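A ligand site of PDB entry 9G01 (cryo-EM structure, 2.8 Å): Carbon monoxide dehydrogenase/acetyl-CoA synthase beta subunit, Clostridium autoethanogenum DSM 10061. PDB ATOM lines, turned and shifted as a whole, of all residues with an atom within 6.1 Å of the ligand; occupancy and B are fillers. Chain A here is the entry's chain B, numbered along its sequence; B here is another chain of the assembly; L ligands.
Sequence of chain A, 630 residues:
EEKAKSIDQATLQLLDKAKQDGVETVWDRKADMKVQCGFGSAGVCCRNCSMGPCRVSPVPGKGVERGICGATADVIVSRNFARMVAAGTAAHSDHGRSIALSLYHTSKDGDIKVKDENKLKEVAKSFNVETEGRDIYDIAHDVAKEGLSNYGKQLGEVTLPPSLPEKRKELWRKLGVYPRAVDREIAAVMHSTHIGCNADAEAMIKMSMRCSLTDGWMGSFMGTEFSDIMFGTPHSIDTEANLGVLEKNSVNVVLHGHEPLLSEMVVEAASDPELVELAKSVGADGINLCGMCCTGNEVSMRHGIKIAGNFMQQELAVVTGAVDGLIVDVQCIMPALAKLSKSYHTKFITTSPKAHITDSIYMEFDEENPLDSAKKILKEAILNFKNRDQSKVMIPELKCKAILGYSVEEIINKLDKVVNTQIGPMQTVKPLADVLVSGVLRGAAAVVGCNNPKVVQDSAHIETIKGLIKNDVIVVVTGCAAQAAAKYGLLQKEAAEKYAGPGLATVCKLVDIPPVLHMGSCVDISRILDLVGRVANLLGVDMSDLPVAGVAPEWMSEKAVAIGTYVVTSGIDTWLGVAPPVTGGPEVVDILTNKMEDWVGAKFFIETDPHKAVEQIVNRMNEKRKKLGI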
ATOM      1  N   HIS A  92      29.146 -16.955  -0.760  1.00  0.00           N
ATOM      2  CA  HIS A  92      29.430 -16.341  -2.059  1.00  0.00           C
ATOM      3  C   HIS A  92      30.412 -17.171  -2.894  1.00  0.00           C
ATOM      4  O   HIS A  92      30.226 -17.333  -4.104  1.00  0.00           O
ATOM      5  CB  HIS A  92      29.954 -14.922  -1.872  1.00  0.00           C
ATOM      6  CG  HIS A  92      28.856 -13.918  -1.626  1.00  0.00           C
ATOM      7  ND1 HIS A  92      29.004 -12.849  -0.775  1.00  0.00           N
ATOM      8  CD2 HIS A  92      27.602 -13.840  -2.113  1.00  0.00           C
ATOM      9  CE1 HIS A  92      27.880 -12.156  -0.742  1.00  0.00           C
ATOM     10  NE2 HIS A  92      27.012 -12.730  -1.565  1.00  0.00           N
ATOM     11  N   GLY A 257      15.912 -17.936  -4.442  1.00  0.00           N
ATOM     12  CA  GLY A 257      17.263 -18.423  -4.219  1.00  0.00           C
ATOM     13  C   GLY A 257      18.339 -17.568  -4.875  1.00  0.00           C
ATOM     14  O   GLY A 257      18.153 -16.363  -5.048  1.00  0.00           O
ATOM     15  N   HIS A 258      19.499 -18.171  -5.182  1.00  0.00           N
ATOM     16  CA  HIS A 258      20.636 -17.395  -5.651  1.00  0.00           C
ATOM     17  C   HIS A 258      21.331 -17.926  -6.903  1.00  0.00           C
ATOM     18  O   HIS A 258      21.865 -17.139  -7.697  1.00  0.00           O
ATOM     19  CB  HIS A 258      21.659 -17.255  -4.513  1.00  0.00           C
ATOM     20  CG  HIS A 258      21.203 -16.315  -3.426  1.00  0.00           C
ATOM     21  ND1 HIS A 258      20.188 -16.617  -2.551  1.00  0.00           N
ATOM     22  CD2 HIS A 258      21.608 -15.058  -3.114  1.00  0.00           C
ATOM     23  CE1 HIS A 258      19.990 -15.601  -1.734  1.00  0.00           C
ATOM     24  NE2 HIS A 258      20.840 -14.631  -2.068  1.00  0.00           N
ATOM     25  N   CYS A 293      14.206 -12.388  -4.663  1.00  0.00           N
ATOM     26  CA  CYS A 293      15.576 -12.261  -4.118  1.00  0.00           C
ATOM     27  C   CYS A 293      16.559 -12.284  -5.295  1.00  0.00           C
ATOM     28  O   CYS A 293      16.268 -11.718  -6.361  1.00  0.00           O
ATOM     29  CB  CYS A 293      15.806 -13.349  -3.068  1.00  0.00           C
ATOM     30  SG  CYS A 293      14.856 -13.154  -1.533  1.00  0.00           S
ATOM     31  N   CYS A 294      17.726 -12.902  -5.121  1.00  0.00           N
ATOM     32  CA  CYS A 294      18.833 -12.732  -6.070  1.00  0.00           C
ATOM     33  C   CYS A 294      18.622 -13.506  -7.358  1.00  0.00           C
ATOM     34  O   CYS A 294      19.040 -13.044  -8.423  1.00  0.00           O
ATOM     35  CB  CYS A 294      20.155 -13.120  -5.422  1.00  0.00           C
ATOM     36  SG  CYS A 294      20.777 -11.819  -4.354  1.00  0.00           S
ATOM     37  N   ASN A 310      11.153  -9.250  -2.403  1.00  0.00           N
ATOM     38  CA  ASN A 310      12.442  -9.477  -1.750  1.00  0.00           C
ATOM     39  C   ASN A 310      12.278 -10.405  -0.540  1.00  0.00           C
ATOM     40  O   ASN A 310      11.236 -11.036  -0.335  1.00  0.00           O
ATOM     41  CB  ASN A 310      13.136  -8.149  -1.410  1.00  0.00           C
ATOM     42  CG  ASN A 310      12.241  -7.147  -0.676  1.00  0.00           C
ATOM     43  OD1 ASN A 310      11.158  -7.500  -0.230  1.00  0.00           O
ATOM     44  ND2 ASN A 310      12.703  -5.899  -0.545  1.00  0.00           N
ATOM     45  N   PHE A 311      13.315 -10.473   0.307  1.00  0.00           N
ATOM     46  CA  PHE A 311      13.456 -11.502   1.342  1.00  0.00           C
ATOM     47  C   PHE A 311      12.193 -11.626   2.197  1.00  0.00           C
ATOM     48  O   PHE A 311      11.567 -12.690   2.200  1.00  0.00           O
ATOM     49  CB  PHE A 311      14.689 -11.198   2.204  1.00  0.00           C
ATOM     50  CG  PHE A 311      14.898 -12.180   3.346  1.00  0.00           C
ATOM     51  CD1 PHE A 311      15.255 -13.513   3.088  1.00  0.00           C
ATOM     52  CD2 PHE A 311      14.752 -11.761   4.667  1.00  0.00           C
ATOM     53  CE1 PHE A 311      15.459 -14.434   4.147  1.00  0.00           C
ATOM     54  CE2 PHE A 311      14.953 -12.662   5.756  1.00  0.00           C
ATOM     55  CZ  PHE A 311      15.309 -14.004   5.487  1.00  0.00           C
ATOM     56  N   GLN A 331      20.218 -20.554  -0.041  1.00  0.00           N
ATOM     57  CA  GLN A 331      20.486 -19.264   0.592  1.00  0.00           C
ATOM     58  C   GLN A 331      19.218 -18.406   0.716  1.00  0.00           C
ATOM     59  O   GLN A 331      18.467 -18.238  -0.251  1.00  0.00           O
ATOM     60  CB  GLN A 331      21.578 -18.479  -0.157  1.00  0.00           C
ATOM     61  CG  GLN A 331      22.956 -19.196  -0.173  1.00  0.00           C
ATOM     62  CD  GLN A 331      24.001 -18.410  -0.979  1.00  0.00           C
ATOM     63  OE1 GLN A 331      23.880 -17.202  -1.146  1.00  0.00           O
ATOM     64  NE2 GLN A 331      25.009 -19.103  -1.501  1.00  0.00           N
ATOM     65  N   CYS A 332      18.976 -17.849   1.908  1.00  0.00           N
ATOM     66  CA  CYS A 332      17.876 -16.910   2.160  1.00  0.00           C
ATOM     67  C   CYS A 332      16.507 -17.506   1.836  1.00  0.00           C
ATOM     68  O   CYS A 332      15.566 -16.791   1.490  1.00  0.00           O
ATOM     69  CB  CYS A 332      18.088 -15.603   1.397  1.00  0.00           C
ATOM     70  SG  CYS A 332      19.722 -14.886   1.705  1.00  0.00           S
ATOM     71  N   VAL A 448      22.676  -1.699  -0.616  1.00  0.00           N
ATOM     72  CA  VAL A 448      22.672  -3.158  -0.723  1.00  0.00           C
ATOM     73  C   VAL A 448      22.081  -3.720   0.563  1.00  0.00           C
ATOM     74  O   VAL A 448      21.894  -3.002   1.548  1.00  0.00           O
ATOM     75  CB  VAL A 448      24.099  -3.720  -0.948  1.00  0.00           C
ATOM     76  CG1 VAL A 448      24.794  -2.957  -2.073  1.00  0.00           C
ATOM     77  CG2 VAL A 448      24.922  -3.635   0.343  1.00  0.00           C
ATOM     78  N   GLY A 449      21.786  -5.011   0.558  1.00  0.00           N
ATOM     79  CA  GLY A 449      21.433  -5.678   1.800  1.00  0.00           C
ATOM     80  C   GLY A 449      20.025  -6.229   1.772  1.00  0.00           C
ATOM     81  O   GLY A 449      19.260  -6.040   0.826  1.00  0.00           O
ATOM     82  N   CYS A 450      19.665  -6.871   2.879  1.00  0.00           N
ATOM     83  CA  CYS A 450      18.431  -7.610   3.035  1.00  0.00           C
ATOM     84  C   CYS A 450      17.356  -6.777   3.719  1.00  0.00           C
ATOM     85  O   CYS A 450      17.462  -5.547   3.800  1.00  0.00           O
ATOM     86  CB  CYS A 450      18.737  -8.823   3.936  1.00  0.00           C
ATOM     87  SG  CYS A 450      20.493  -9.319   3.953  1.00  0.00           S
ATOM     88  N   ASN A 451      16.296  -7.435   4.156  1.00  0.00           N
ATOM     89  CA  ASN A 451      15.351  -6.893   5.111  1.00  0.00           C
ATOM     90  C   ASN A 451      15.700  -7.490   6.474  1.00  0.00           C
ATOM     91  O   ASN A 451      16.490  -8.439   6.574  1.00  0.00           O
ATOM     92  CB  ASN A 451      13.901  -7.217   4.741  1.00  0.00           C
ATOM     93  CG  ASN A 451      13.511  -6.709   3.364  1.00  0.00           C
ATOM     94  OD1 ASN A 451      13.019  -7.467   2.538  1.00  0.00           O
ATOM     95  ND2 ASN A 451      13.745  -5.402   3.112  1.00  0.00           N
ATOM     96  N   THR A 478      21.624  -3.073  -5.258  1.00  0.00           N
ATOM     97  CA  THR A 478      21.679  -4.508  -5.519  1.00  0.00           C
ATOM     98  C   THR A 478      20.755  -5.242  -4.546  1.00  0.00           C
ATOM     99  O   THR A 478      20.389  -4.718  -3.491  1.00  0.00           O
ATOM    100  CB  THR A 478      23.097  -5.107  -5.417  1.00  0.00           C
ATOM    101  OG1 THR A 478      23.568  -5.051  -4.058  1.00  0.00           O
ATOM    102  CG2 THR A 478      24.068  -4.373  -6.333  1.00  0.00           C
ATOM    103  N   GLY A 479      20.362  -6.442  -4.941  1.00  0.00           N
ATOM    104  CA  GLY A 479      19.687  -7.350  -4.023  1.00  0.00           C
ATOM    105  C   GLY A 479      18.315  -6.894  -3.569  1.00  0.00           C
ATOM    106  O   GLY A 479      17.528  -6.300  -4.322  1.00  0.00           O
ATOM    107  N   CYS A 480      18.028  -7.191  -2.300  1.00  0.00           N
ATOM    108  CA  CYS A 480      16.709  -6.885  -1.755  1.00  0.00           C
ATOM    109  C   CYS A 480      16.474  -5.380  -1.649  1.00  0.00           C
ATOM    110  O   CYS A 480      15.334  -4.927  -1.770  1.00  0.00           O
ATOM    111  CB  CYS A 480      16.556  -7.581  -0.394  1.00  0.00           C
ATOM    112  SG  CYS A 480      16.330  -9.395  -0.588  1.00  0.00           S
ATOM    113  N   ALA A 481      17.535  -4.588  -1.441  1.00  0.00           N
ATOM    114  CA  ALA A 481      17.409  -3.133  -1.520  1.00  0.00           C
ATOM    115  C   ALA A 481      16.996  -2.687  -2.909  1.00  0.00           C
ATOM    116  O   ALA A 481      16.090  -1.848  -3.067  1.00  0.00           O
ATOM    117  CB  ALA A 481      18.726  -2.470  -1.114  1.00  0.00           C
ATOM    118  N   GLN A 483      15.315  -4.459  -4.996  1.00  0.00           N
ATOM    119  CA  GLN A 483      13.914  -4.858  -5.162  1.00  0.00           C
ATOM    120  C   GLN A 483      12.971  -3.949  -4.385  1.00  0.00           C
ATOM    121  O   GLN A 483      11.873  -3.645  -4.856  1.00  0.00           O
ATOM    122  CB  GLN A 483      13.757  -6.338  -4.796  1.00  0.00           C
ATOM    123  CG  GLN A 483      14.512  -7.252  -5.811  1.00  0.00           C
ATOM    124  CD  GLN A 483      14.516  -8.751  -5.454  1.00  0.00           C
ATOM    125  OE1 GLN A 483      14.305  -9.119  -4.313  1.00  0.00           O
ATOM    126  NE2 GLN A 483      14.771  -9.602  -6.454  1.00  0.00           N
ATOM    127  N   SER A 521      22.298  -8.705  -8.594  1.00  0.00           N
ATOM    128  CA  SER A 521      22.166  -9.474  -7.359  1.00  0.00           C
ATOM    129  C   SER A 521      23.281  -9.108  -6.384  1.00  0.00           C
ATOM    130  O   SER A 521      24.051  -8.184  -6.597  1.00  0.00           O
ATOM    131  CB  SER A 521      22.150 -10.971  -7.687  1.00  0.00           C
ATOM    132  OG  SER A 521      23.392 -11.399  -8.225  1.00  0.00           O
ATOM    133  N   CYS A 522      23.363  -9.867  -5.280  1.00  0.00           N
ATOM    134  CA  CYS A 522      24.377  -9.598  -4.259  1.00  0.00           C
ATOM    135  C   CYS A 522      25.782  -9.852  -4.785  1.00  0.00           C
ATOM    136  O   CYS A 522      26.705  -9.075  -4.518  1.00  0.00           O
ATOM    137  CB  CYS A 522      24.076 -10.420  -3.012  1.00  0.00           C
ATOM    138  SG  CYS A 522      22.616  -9.774  -2.187  1.00  0.00           S
ATOM    139  N   MET A 556      20.682  -8.559   7.180  1.00  0.00           N
ATOM    140  CA  MET A 556      20.482  -9.651   8.126  1.00  0.00           C
ATOM    141  C   MET A 556      21.509 -10.780   8.015  1.00  0.00           C
ATOM    142  O   MET A 556      21.814 -11.424   9.014  1.00  0.00           O
ATOM    143  CB  MET A 556      19.050 -10.205   7.996  1.00  0.00           C
ATOM    144  CG  MET A 556      18.776 -10.998   6.695  1.00  0.00           C
ATOM    145  SD  MET A 556      19.158 -12.771   6.740  1.00  0.00           S
ATOM    146  CE  MET A 556      18.847 -13.252   5.040  1.00  0.00           C
ATOM    147  N   SER A 557      22.053 -11.026   6.816  1.00  0.00           N
ATOM    148  CA  SER A 557      22.779 -12.254   6.529  1.00  0.00           C
ATOM    149  C   SER A 557      24.267 -12.129   6.832  1.00  0.00           C
ATOM    150  O   SER A 557      24.846 -11.035   6.875  1.00  0.00           O
ATOM    151  CB  SER A 557      22.589 -12.682   5.056  1.00  0.00           C
ATOM    152  OG  SER A 557      23.164 -11.745   4.149  1.00  0.00           O
ATOM    153  N   LYS A 559      26.357 -13.093   4.689  1.00  0.00           N
ATOM    154  CA  LYS A 559      26.845 -12.550   3.424  1.00  0.00           C
ATOM    155  C   LYS A 559      26.938 -11.024   3.474  1.00  0.00           C
ATOM    156  O   LYS A 559      27.945 -10.459   3.027  1.00  0.00           O
ATOM    157  CB  LYS A 559      25.932 -12.968   2.278  1.00  0.00           C
ATOM    158  CG  LYS A 559      26.190 -14.395   1.756  1.00  0.00           C
ATOM    159  CD  LYS A 559      25.245 -14.736   0.591  1.00  0.00           C
ATOM    160  CE  LYS A 559      23.767 -14.853   1.074  1.00  0.00           C
ATOM    161  NZ  LYS A 559      22.770 -15.040  -0.058  1.00  0.00           N
ATOM    162  N   ALA A 560      25.972 -10.360   4.094  1.00  0.00           N
ATOM    163  CA  ALA A 560      26.026  -8.908   4.225  1.00  0.00           C
ATOM    164  C   ALA A 560      27.227  -8.472   5.052  1.00  0.00           C
ATOM    165  O   ALA A 560      27.884  -7.469   4.739  1.00  0.00           O
ATOM    166  CB  ALA A 560      24.726  -8.385   4.833  1.00  0.00           C
ATOM    167  N   ILE A 563      30.245  -8.756   2.872  1.00  0.00           N
ATOM    168  CA  ILE A 563      30.197  -7.699   1.855  1.00  0.00           C
ATOM    169  C   ILE A 563      30.671  -6.379   2.433  1.00  0.00           C
ATOM    170  O   ILE A 563      31.547  -5.704   1.866  1.00  0.00           O
ATOM    171  CB  ILE A 563      28.784  -7.569   1.268  1.00  0.00           C
ATOM    172  CG1 ILE A 563      28.463  -8.740   0.342  1.00  0.00           C
ATOM    173  CG2 ILE A 563      28.604  -6.220   0.513  1.00  0.00           C
ATOM    174  CD1 ILE A 563      26.979  -8.874   0.081  1.00  0.00           C
ATOM    175  N   HIS B 194      24.567 -21.378   6.486  1.00  0.00           N
ATOM    176  CA  HIS B 194      24.108 -20.001   6.327  1.00  0.00           C
ATOM    177  C   HIS B 194      22.589 -19.913   6.377  1.00  0.00           C
ATOM    178  O   HIS B 194      21.884 -20.846   5.991  1.00  0.00           O
ATOM    179  CB  HIS B 194      24.638 -19.455   4.991  1.00  0.00           C
ATOM    180  CG  HIS B 194      24.339 -18.013   4.749  1.00  0.00           C
ATOM    181  ND1 HIS B 194      23.101 -17.553   4.349  1.00  0.00           N
ATOM    182  CD2 HIS B 194      25.126 -16.907   4.843  1.00  0.00           C
ATOM    183  CE1 HIS B 194      23.129 -16.245   4.218  1.00  0.00           C
ATOM    184  NE2 HIS B 194      24.358 -15.823   4.509  1.00  0.00           N
HETATM  185 FE1  LIG L   1      19.567 -12.691   0.898  1.00  0.00          FE
HETATM  186 FE2  LIG L   1      20.891 -12.572  -2.211  1.00  0.00          FE
HETATM  187 FE3  LIG L   1      20.181 -10.290   1.859  1.00  0.00          FE
HETATM  188 FE4  LIG L   1      18.250 -10.367  -0.088  1.00  0.00          FE
HETATM  189  S1  LIG L   1      20.210  -9.132  -0.117  1.00  0.00           S
HETATM  190  S2  LIG L   1      18.132 -11.255   2.060  1.00  0.00           S
HETATM  191  S3  LIG L   1      21.729 -12.005   1.449  1.00  0.00           S
HETATM  192  S4  LIG L   1      18.802 -12.375  -1.177  1.00  0.00           S
HETATM  193 NI1  LIG L   1      21.700 -10.814  -0.624  1.00  0.00          NI
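A sulfur (S3) of the ligand sits close to the side-chain amino group (NZ) of Lys 559 (3.5 Å). The backbone NH (N) of Cys 480 sits close to a sulfur (S1) of the ligand, at 3.6 Å. The side-chain sulfur (SG) of Cys 450 binds an iron atom (FE3) of the ligand (2.3 Å). The side-chain sulfur (SG) of Cys 294 is bound to an iron atom (FE2) of the ligand (2.3 Å). A nickel atom (NI1) of the ligand is bound by the side-chain sulfur (SG) of Cys 522 (2.1 Å). SG of Cys 480 is bound to FE4 of the ligand, 2.2 Å away. An iron atom (FE1) of the ligand is bound by the side-chain sulfur (SG) of Cys 332, 2.3 Å away. An iron atom (FE2) of the ligand is bound by a ring nitrogen (NE2) of His 258 (2.1 Å). A sulfur (S3) of the ligand lies close to the side-chain hydroxyl (OG) of Ser 557, at 3.1 Å. S1 of the ligand lies close to N of Cys 450.
The backbone NH (N) of Ala 560 sits at hydrogen-bond distance from the side-chain hydroxyl (OG) of Ser 557 (3.1 Å). The backbone NH (N) of Ala 481 is in hydrogen-bond range of the backbone carbonyl oxygen (O) of Gly 449 (3.2 Å). NZ of Lys 559 sits close to SG of Cys 332 (3.5 Å). The side-chain sulfur (SG) of Cys 450 sits close to the side-chain hydroxyl (OG) of Ser 557 (3.6 Å). NE2 of Gln 483 is in hydrogen-bond range of O of Cys 293, at 2.6 Å. OE1 of Gln 331 lies within hydrogen-bond range of NZ of Lys 559 (2.7 Å). NE2 of His 258 sits close to NZ of Lys 559, at 2.8 Å. A ring nitrogen (NE2) of His 194 of chain B sits at hydrogen-bond distance from the backbone NH (N) of Lys 559.
A sulfur (S1) of the ligand sits close to the backbone carbonyl oxygen (O) of Gly 449, 3.4 Å away. CB of Cys 293 touches S4 of the ligand (3.7 Å). Phe 311 touches the ligand (CB to S2, 3.4 Å). CE of Met 556 touches S2 of the ligand (3.7 Å). Of the 26 residues printed, 12 come within 4 Å of the ligand.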
